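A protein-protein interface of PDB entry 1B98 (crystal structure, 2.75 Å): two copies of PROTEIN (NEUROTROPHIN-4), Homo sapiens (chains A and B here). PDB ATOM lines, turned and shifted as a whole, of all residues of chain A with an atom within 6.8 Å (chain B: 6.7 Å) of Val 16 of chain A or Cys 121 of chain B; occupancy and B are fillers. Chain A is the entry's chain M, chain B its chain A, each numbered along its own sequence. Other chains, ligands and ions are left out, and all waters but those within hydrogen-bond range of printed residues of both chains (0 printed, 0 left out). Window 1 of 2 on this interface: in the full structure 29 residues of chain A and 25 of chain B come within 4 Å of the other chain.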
ATOM      1  N   LEU A  14     -12.983  -7.354  34.076  1.00  0.00           N
ATOM      2  CA  LEU A  14     -13.779  -6.220  33.676  1.00  0.00           C
ATOM      3  C   LEU A  14     -13.106  -5.474  32.516  1.00  0.00           C
ATOM      4  O   LEU A  14     -11.893  -5.264  32.507  1.00  0.00           O
ATOM      5  CB  LEU A  14     -14.021  -5.264  34.823  1.00  0.00           C
ATOM      6  CG  LEU A  14     -14.878  -5.569  36.027  1.00  0.00           C
ATOM      7  CD1 LEU A  14     -15.127  -4.232  36.741  1.00  0.00           C
ATOM      8  CD2 LEU A  14     -16.200  -6.226  35.658  1.00  0.00           C
ATOM      9  N   ALA A  15     -13.901  -5.041  31.545  1.00  0.00           N
ATOM     10  CA  ALA A  15     -13.311  -4.162  30.526  1.00  0.00           C
ATOM     11  C   ALA A  15     -13.139  -2.735  31.095  1.00  0.00           C
ATOM     12  O   ALA A  15     -13.912  -2.234  31.906  1.00  0.00           O
ATOM     13  CB  ALA A  15     -14.203  -4.031  29.309  1.00  0.00           C
ATOM     14  N   VAL A  16     -12.158  -2.046  30.580  1.00  0.00           N
ATOM     15  CA  VAL A  16     -11.887  -0.638  30.852  1.00  0.00           C
ATOM     16  C   VAL A  16     -12.922   0.223  30.128  1.00  0.00           C
ATOM     17  O   VAL A  16     -13.430   1.245  30.633  1.00  0.00           O
ATOM     18  CB  VAL A  16     -10.412  -0.547  30.442  1.00  0.00           C
ATOM     19  CG1 VAL A  16     -10.205   0.277  29.195  1.00  0.00           C
ATOM     20  CG2 VAL A  16      -9.516  -0.249  31.608  1.00  0.00           C
ATOM     21  N   CYS A  17     -13.352  -0.146  28.949  1.00  0.00           N
ATOM     22  CA  CYS A  17     -14.386   0.520  28.173  1.00  0.00           C
ATOM     23  C   CYS A  17     -15.340  -0.592  27.745  1.00  0.00           C
ATOM     24  O   CYS A  17     -14.919  -1.702  27.330  1.00  0.00           O
ATOM     25  CB  CYS A  17     -13.882   1.270  26.927  1.00  0.00           C
ATOM     26  SG  CYS A  17     -12.820   2.697  27.362  1.00  0.00           S
ATOM     27  N   ASP A  18     -16.612  -0.339  28.012  1.00  0.00           N
ATOM     28  CA  ASP A  18     -17.611  -1.331  27.641  1.00  0.00           C
ATOM     29  C   ASP A  18     -17.806  -1.353  26.124  1.00  0.00           C
ATOM     30  O   ASP A  18     -17.851  -0.284  25.450  1.00  0.00           O
ATOM     31  CB  ASP A  18     -18.953  -1.035  28.319  1.00  0.00           C
ATOM     32  CG  ASP A  18     -18.970  -1.224  29.829  1.00  0.00           C
ATOM     33  OD1 ASP A  18     -18.242  -2.143  30.264  1.00  0.00           O
ATOM     34  OD2 ASP A  18     -19.684  -0.443  30.504  1.00  0.00           O
ATOM     35  N   PRO A  71     -18.536   5.242  34.990  1.00  0.00           N
ATOM     36  CA  PRO A  71     -17.736   5.261  33.788  1.00  0.00           C
ATOM     37  C   PRO A  71     -17.756   3.993  32.927  1.00  0.00           C
ATOM     38  O   PRO A  71     -18.543   3.071  33.053  1.00  0.00           O
ATOM     39  CB  PRO A  71     -16.282   5.476  34.251  1.00  0.00           C
ATOM     40  CG  PRO A  71     -16.314   5.583  35.717  1.00  0.00           C
ATOM     41  CD  PRO A  71     -17.656   5.100  36.184  1.00  0.00           C
ATOM     42  N   GLY A  72     -16.821   3.947  31.985  1.00  0.00           N
ATOM     43  CA  GLY A  72     -16.552   2.928  31.013  1.00  0.00           C
ATOM     44  C   GLY A  72     -17.532   2.862  29.851  1.00  0.00           C
ATOM     45  O   GLY A  72     -17.820   1.804  29.313  1.00  0.00           O
ATOM     46  N   ALA A  73     -18.126   4.011  29.524  1.00  0.00           N
ATOM     47  CA  ALA A  73     -19.122   4.137  28.479  1.00  0.00           C
ATOM     48  C   ALA A  73     -18.681   5.096  27.395  1.00  0.00           C
ATOM     49  O   ALA A  73     -17.777   5.921  27.633  1.00  0.00           O
ATOM     50  CB  ALA A  73     -20.429   4.632  29.091  1.00  0.00           C
ATOM     51  N   GLY A  77     -15.029   8.717  30.763  1.00  0.00           N
ATOM     52  CA  GLY A  77     -13.738   8.294  31.255  1.00  0.00           C
ATOM     53  C   GLY A  77     -13.716   6.743  31.304  1.00  0.00           C
ATOM     54  O   GLY A  77     -14.773   6.123  31.379  1.00  0.00           O
ATOM     55  N   CYS A  78     -12.501   6.195  31.338  1.00  0.00           N
ATOM     56  CA  CYS A  78     -12.480   4.723  31.313  1.00  0.00           C
ATOM     57  C   CYS A  78     -12.432   4.149  32.722  1.00  0.00           C
ATOM     58  O   CYS A  78     -12.136   4.792  33.702  1.00  0.00           O
ATOM     59  CB  CYS A  78     -11.339   4.184  30.450  1.00  0.00           C
ATOM     60  SG  CYS A  78     -11.030   5.220  28.980  1.00  0.00           S
ATOM     61  N   ARG A  79     -12.834   2.882  32.834  1.00  0.00           N
ATOM     62  CA  ARG A  79     -12.734   2.167  34.078  1.00  0.00           C
ATOM     63  C   ARG A  79     -11.292   1.958  34.533  1.00  0.00           C
ATOM     64  O   ARG A  79     -10.422   1.697  33.712  1.00  0.00           O
ATOM     65  CB  ARG A  79     -13.309   0.783  33.764  1.00  0.00           C
ATOM     66  CG  ARG A  79     -13.984   0.177  34.978  1.00  0.00           C
ATOM     67  CD  ARG A  79     -15.024  -0.760  34.496  1.00  0.00           C
ATOM     68  NE  ARG A  79     -16.394  -0.455  34.311  1.00  0.00           N
ATOM     69  CZ  ARG A  79     -17.048  -0.956  33.241  1.00  0.00           C
ATOM     70  NH1 ARG A  79     -16.311  -1.648  32.355  1.00  0.00           N
ATOM     71  NH2 ARG A  79     -18.344  -0.770  33.026  1.00  0.00           N
ATOM     72  N   GLY A  80     -11.044   2.058  35.869  1.00  0.00           N
ATOM     73  CA  GLY A  80      -9.749   1.788  36.424  1.00  0.00           C
ATOM     74  C   GLY A  80      -8.611   2.728  36.094  1.00  0.00           C
ATOM     75  O   GLY A  80      -7.497   2.413  36.490  1.00  0.00           O
ATOM     76  N   VAL A  81      -8.831   3.846  35.404  1.00  0.00           N
ATOM     77  CA  VAL A  81      -7.718   4.736  35.108  1.00  0.00           C
ATOM     78  C   VAL A  81      -7.511   5.645  36.322  1.00  0.00           C
ATOM     79  O   VAL A  81      -8.477   6.149  36.892  1.00  0.00           O
ATOM     80  CB  VAL A  81      -7.647   5.591  33.827  1.00  0.00           C
ATOM     81  CG1 VAL A  81      -8.146   4.863  32.585  1.00  0.00           C
ATOM     82  CG2 VAL A  81      -8.260   6.976  33.962  1.00  0.00           C
ATOM     83  N   CYS A  90     -13.099   6.545  26.351  1.00  0.00           N
ATOM     84  CA  CYS A  90     -13.547   5.413  25.626  1.00  0.00           C
ATOM     85  C   CYS A  90     -14.060   5.861  24.238  1.00  0.00           C
ATOM     86  O   CYS A  90     -14.975   6.696  24.136  1.00  0.00           O
ATOM     87  CB  CYS A  90     -14.734   4.767  26.379  1.00  0.00           C
ATOM     88  SG  CYS A  90     -14.167   4.030  27.962  1.00  0.00           S
ATOM     89  N   CYS A 119     -13.877  -0.770  21.084  1.00  0.00           N
ATOM     90  CA  CYS A 119     -14.035   0.414  21.891  1.00  0.00           C
ATOM     91  C   CYS A 119     -12.779   0.606  22.756  1.00  0.00           C
ATOM     92  O   CYS A 119     -12.574  -0.286  23.569  1.00  0.00           O
ATOM     93  CB  CYS A 119     -15.266   0.284  22.795  1.00  0.00           C
ATOM     94  SG  CYS A 119     -15.347   1.745  23.867  1.00  0.00           S
ATOM     95  N   VAL A 120     -11.841   1.511  22.598  1.00  0.00           N
ATOM     96  CA  VAL A 120     -10.588   1.531  23.326  1.00  0.00           C
ATOM     97  C   VAL A 120     -10.478   2.753  24.222  1.00  0.00           C
ATOM     98  O   VAL A 120     -11.083   3.801  24.005  1.00  0.00           O
ATOM     99  CB  VAL A 120      -9.288   1.390  22.494  1.00  0.00           C
ATOM    100  CG1 VAL A 120      -9.305   0.192  21.544  1.00  0.00           C
ATOM    101  CG2 VAL A 120      -8.939   2.614  21.694  1.00  0.00           C
ATOM    102  N   CYS A 121      -9.737   2.634  25.294  1.00  0.00           N
ATOM    103  CA  CYS A 121      -9.569   3.695  26.276  1.00  0.00           C
ATOM    104  C   CYS A 121      -8.462   4.629  25.798  1.00  0.00           C
ATOM    105  O   CYS A 121      -7.314   4.230  25.721  1.00  0.00           O
ATOM    106  CB  CYS A 121      -9.217   3.124  27.638  1.00  0.00           C
ATOM    107  SG  CYS A 121      -8.793   4.534  28.738  1.00  0.00           S
ATOM    108  N   VAL B  16      -4.047   3.354  26.217  1.00  0.00           N
ATOM    109  CA  VAL B  16      -3.730   2.490  27.357  1.00  0.00           C
ATOM    110  C   VAL B  16      -2.951   1.272  26.944  1.00  0.00           C
ATOM    111  O   VAL B  16      -2.110   0.795  27.709  1.00  0.00           O
ATOM    112  CB  VAL B  16      -5.173   2.313  27.872  1.00  0.00           C
ATOM    113  CG1 VAL B  16      -5.462   0.873  28.119  1.00  0.00           C
ATOM    114  CG2 VAL B  16      -5.390   3.357  28.968  1.00  0.00           C
ATOM    115  N   CYS B  17      -3.178   0.760  25.741  1.00  0.00           N
ATOM    116  CA  CYS B  17      -2.373  -0.376  25.202  1.00  0.00           C
ATOM    117  C   CYS B  17      -1.894   0.177  23.849  1.00  0.00           C
ATOM    118  O   CYS B  17      -2.620   0.971  23.238  1.00  0.00           O
ATOM    119  CB  CYS B  17      -3.203  -1.627  25.162  1.00  0.00           C
ATOM    120  SG  CYS B  17      -3.691  -2.243  26.806  1.00  0.00           S
ATOM    121  N   GLY B  76       1.527  -6.922  29.398  1.00  0.00           N
ATOM    122  CA  GLY B  76       1.852  -6.077  30.467  1.00  0.00           C
ATOM    123  C   GLY B  76       0.671  -5.232  30.982  1.00  0.00           C
ATOM    124  O   GLY B  76      -0.434  -5.253  30.439  1.00  0.00           O
ATOM    125  N   GLY B  77       0.932  -4.585  32.119  1.00  0.00           N
ATOM    126  CA  GLY B  77       0.021  -3.719  32.802  1.00  0.00           C
ATOM    127  C   GLY B  77      -0.254  -2.514  31.863  1.00  0.00           C
ATOM    128  O   GLY B  77       0.694  -2.046  31.263  1.00  0.00           O
ATOM    129  N   CYS B  78      -1.475  -2.061  31.788  1.00  0.00           N
ATOM    130  CA  CYS B  78      -1.870  -1.016  30.904  1.00  0.00           C
ATOM    131  C   CYS B  78      -1.460   0.382  31.330  1.00  0.00           C
ATOM    132  O   CYS B  78      -1.430   0.655  32.512  1.00  0.00           O
ATOM    133  CB  CYS B  78      -3.398  -1.026  30.768  1.00  0.00           C
ATOM    134  SG  CYS B  78      -4.091  -2.664  30.453  1.00  0.00           S
ATOM    135  N   ARG B  79      -0.995   1.195  30.371  1.00  0.00           N
ATOM    136  CA  ARG B  79      -0.706   2.567  30.684  1.00  0.00           C
ATOM    137  C   ARG B  79      -1.967   3.224  31.306  1.00  0.00           C
ATOM    138  O   ARG B  79      -3.158   3.045  31.040  1.00  0.00           O
ATOM    139  CB  ARG B  79      -0.369   3.395  29.441  1.00  0.00           C
ATOM    140  CG  ARG B  79       0.441   4.628  29.874  1.00  0.00           C
ATOM    141  CD  ARG B  79       0.741   5.439  28.607  1.00  0.00           C
ATOM    142  NE  ARG B  79       1.724   4.803  27.769  1.00  0.00           N
ATOM    143  CZ  ARG B  79       1.759   4.107  26.662  1.00  0.00           C
ATOM    144  NH1 ARG B  79       0.711   3.796  25.886  1.00  0.00           N
ATOM    145  NH2 ARG B  79       2.963   3.714  26.244  1.00  0.00           N
ATOM    146  N   VAL B  81      -3.594   2.832  34.118  1.00  0.00           N
ATOM    147  CA  VAL B  81      -4.501   2.360  35.149  1.00  0.00           C
ATOM    148  C   VAL B  81      -3.921   2.592  36.540  1.00  0.00           C
ATOM    149  O   VAL B  81      -2.720   2.633  36.708  1.00  0.00           O
ATOM    150  CB  VAL B  81      -5.177   0.986  35.077  1.00  0.00           C
ATOM    151  CG1 VAL B  81      -5.238   0.469  33.645  1.00  0.00           C
ATOM    152  CG2 VAL B  81      -4.748  -0.033  36.089  1.00  0.00           C
ATOM    153  N   SER B  88      -4.000  -5.033  35.593  1.00  0.00           N
ATOM    154  CA  SER B  88      -4.429  -4.955  34.209  1.00  0.00           C
ATOM    155  C   SER B  88      -3.455  -5.658  33.268  1.00  0.00           C
ATOM    156  O   SER B  88      -2.373  -6.066  33.676  1.00  0.00           O
ATOM    157  CB  SER B  88      -4.724  -3.507  33.859  1.00  0.00           C
ATOM    158  OG  SER B  88      -3.522  -2.763  33.669  1.00  0.00           O
ATOM    159  N   GLU B  89      -3.910  -5.825  32.031  1.00  0.00           N
ATOM    160  CA  GLU B  89      -3.230  -6.485  30.950  1.00  0.00           C
ATOM    161  C   GLU B  89      -3.707  -6.075  29.533  1.00  0.00           C
ATOM    162  O   GLU B  89      -4.908  -6.127  29.242  1.00  0.00           O
ATOM    163  CB  GLU B  89      -3.420  -8.010  31.033  1.00  0.00           C
ATOM    164  CG  GLU B  89      -2.618  -8.782  29.997  1.00  0.00           C
ATOM    165  CD  GLU B  89      -2.805 -10.305  30.079  1.00  0.00           C
ATOM    166  OE1 GLU B  89      -3.877 -10.884  29.796  1.00  0.00           O
ATOM    167  OE2 GLU B  89      -1.818 -10.964  30.433  1.00  0.00           O
ATOM    168  N   CYS B  90      -2.749  -5.650  28.708  1.00  0.00           N
ATOM    169  CA  CYS B  90      -2.971  -5.419  27.285  1.00  0.00           C
ATOM    170  C   CYS B  90      -3.002  -6.776  26.591  1.00  0.00           C
ATOM    171  O   CYS B  90      -2.093  -7.579  26.832  1.00  0.00           O
ATOM    172  CB  CYS B  90      -1.889  -4.556  26.695  1.00  0.00           C
ATOM    173  SG  CYS B  90      -1.917  -2.916  27.495  1.00  0.00           S
ATOM    174  N   LYS B  91      -4.088  -7.069  25.914  1.00  0.00           N
ATOM    175  CA  LYS B  91      -4.274  -8.344  25.239  1.00  0.00           C
ATOM    176  C   LYS B  91      -4.820  -8.068  23.837  1.00  0.00           C
ATOM    177  O   LYS B  91      -5.459  -6.998  23.666  1.00  0.00           O
ATOM    178  CB  LYS B  91      -5.316  -9.140  25.975  1.00  0.00           C
ATOM    179  CG  LYS B  91      -4.954 -10.337  26.804  1.00  0.00           C
ATOM    180  CD  LYS B  91      -6.141 -10.845  27.611  1.00  0.00           C
ATOM    181  CE  LYS B  91      -6.310  -9.859  28.807  1.00  0.00           C
ATOM    182  NZ  LYS B  91      -6.475 -10.740  30.030  1.00  0.00           N
ATOM    183  N   CYS B 119      -5.576  -4.008  20.403  1.00  0.00           N
ATOM    184  CA  CYS B 119      -4.924  -4.286  21.648  1.00  0.00           C
ATOM    185  C   CYS B 119      -5.777  -3.584  22.699  1.00  0.00           C
ATOM    186  O   CYS B 119      -5.897  -2.365  22.755  1.00  0.00           O
ATOM    187  CB  CYS B 119      -3.447  -3.815  21.677  1.00  0.00           C
ATOM    188  SG  CYS B 119      -2.579  -4.389  23.178  1.00  0.00           S
ATOM    189  N   VAL B 120      -6.523  -4.322  23.535  1.00  0.00           N
ATOM    190  CA  VAL B 120      -7.410  -3.648  24.478  1.00  0.00           C
ATOM    191  C   VAL B 120      -6.962  -3.936  25.907  1.00  0.00           C
ATOM    192  O   VAL B 120      -6.370  -4.984  26.152  1.00  0.00           O
ATOM    193  CB  VAL B 120      -8.852  -4.134  24.266  1.00  0.00           C
ATOM    194  CG1 VAL B 120      -9.298  -4.009  22.831  1.00  0.00           C
ATOM    195  CG2 VAL B 120      -8.946  -5.621  24.610  1.00  0.00           C
ATOM    196  N   CYS B 121      -7.236  -3.068  26.848  1.00  0.00           N
ATOM    197  CA  CYS B 121      -6.776  -3.366  28.200  1.00  0.00           C
ATOM    198  C   CYS B 121      -7.800  -4.121  29.012  1.00  0.00           C
ATOM    199  O   CYS B 121      -8.920  -3.592  29.025  1.00  0.00           O
ATOM    200  CB  CYS B 121      -6.530  -2.009  28.874  1.00  0.00           C
ATOM    201  SG  CYS B 121      -6.087  -2.092  30.586  1.00  0.00           S
ATOM    202  N   THR B 122      -7.441  -5.170  29.756  1.00  0.00           N
ATOM    203  CA  THR B 122      -8.451  -5.777  30.650  1.00  0.00           C
ATOM    204  C   THR B 122      -7.985  -5.616  32.112  1.00  0.00           C
ATOM    205  O   THR B 122      -6.863  -5.891  32.467  1.00  0.00           O
ATOM    206  CB  THR B 122      -8.738  -7.295  30.595  1.00  0.00           C
ATOM    207  OG1 THR B 122      -8.748  -7.836  29.281  1.00  0.00           O
ATOM    208  CG2 THR B 122     -10.085  -7.605  31.245  1.00  0.00           C
ATOM    209  N   LEU B 123      -8.920  -5.333  32.961  1.00  0.00           N
ATOM    210  CA  LEU B 123      -8.822  -5.253  34.402  1.00  0.00           C
ATOM    211  C   LEU B 123      -9.294  -6.649  34.839  1.00  0.00           C
ATOM    212  O   LEU B 123     -10.462  -6.958  34.729  1.00  0.00           O
ATOM    213  CB  LEU B 123      -9.800  -4.236  34.993  1.00  0.00           C
ATOM    214  CG  LEU B 123      -9.796  -2.874  34.292  1.00  0.00           C
ATOM    215  CD1 LEU B 123     -11.026  -2.073  34.666  1.00  0.00           C
ATOM    216  CD2 LEU B 123      -8.541  -2.089  34.675  1.00  0.00           C
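O of Leu 123 of chain B is in hydrogen-bond range of N of Leu 14 of chain A (2.6 Å).
N of Val 16 of chain B sits at hydrogen-bond distance from O of Cys 121 of chain A (3.4 Å).
The side-chain sulfur (SG) of Cys 17 of chain B sits close to the backbone NH (N) of Cys 121 of chain B, 3.6 Å away.
The side-chain sulfur (SG) of Cys 17 of chain A is disulfide-bonded to the side-chain sulfur (SG) of Cys 90 of chain A (2.0 Å).
The backbone carbonyl oxygen of Glu 89 of chain B is in hydrogen-bond range of the backbone NH of Thr 122 of chain B (2.8 Å).
O of Ala 15 of chain A is in hydrogen-bond range of NH1 of Arg 79 of chain A (2.5 Å).
SG of Cys 90 of chain B is disulfide-bonded to SG of Cys 17 of chain B, 2.0 Å away.
The side-chain sulfur of Cys 121 of chain B is disulfide-bonded to the side-chain sulfur of Cys 78 of chain B, at 2.1 Å.
Among the printed residues, pairs that only touch across the chains: Gly 80 of chain A with Val 81 of chain B (3.1 Å), Leu 14 of chain A with Thr 122 of chain B (3.2 Å), Val 16 of chain A with Cys 121 of chain B (3.7 Å), Val 16 of chain A with Leu 123 of chain B (3.7 Å), Arg 79 of chain A with Leu 123 of chain B (3.7 Å), Ala 15 of chain A with Leu 123 of chain B (3.997 Å) and Val 81 of chain A with Val 81 of chain B (3.9995 Å).
Val 16 of chain A touches just these residues of chain B: Cys 121 and Leu 123.
Cys 121 of chain B touches one residue of chain A.
Of the printed residues of chain B, Cys 121 of chain A touches Val 16 (3.4 Å).
Printed residues of chain A within 4 Å of Leu 123 of chain B: Leu 14 (2.6 Å), Ala 15 (3.997 Å), Val 16 (3.7 Å) and Arg 79 (3.7 Å).
Of the printed residues of chain B, Ala 15 of chain A touches Leu 123.
Of the printed residues of chain A, Val 81 of chain B touches Gly 80 (3.1 Å) and Val 81 (3.9995 Å).
Hydrophobic or aromatic side chains of chain B within 4 Å of the printed part of chain A: Val 16, Val 81 and Leu 123.
Along chain B the printed residues that touch a printed residue of chain A span positions 16 to 123.
Printed residues of chain A that touch a printed residue of chain B: Leu 14, Ala 15, Val 16, Arg 79, Gly 80, Val 81 and Cys 121.
Hydrophobic or aromatic side chains of chain A that line the printed part of chain B: Leu 14 and Val 16.
Among the printed residues, no Asp or Glu carboxylate lies within 4 Å of a Lys or Arg side-chain nitrogen of the other chain.
Val 16 of chain A touches Cys 121 of chain B, and with the chains exchanged Cys 121 of chain A touches Val 16 of chain B.
Val 81 of chain B touches its own counterpart, Val 81 of chain A.
Of the 9 pairs that touch across the chains among the printed residues, 3 have their exchanged pair printed and touching as well.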
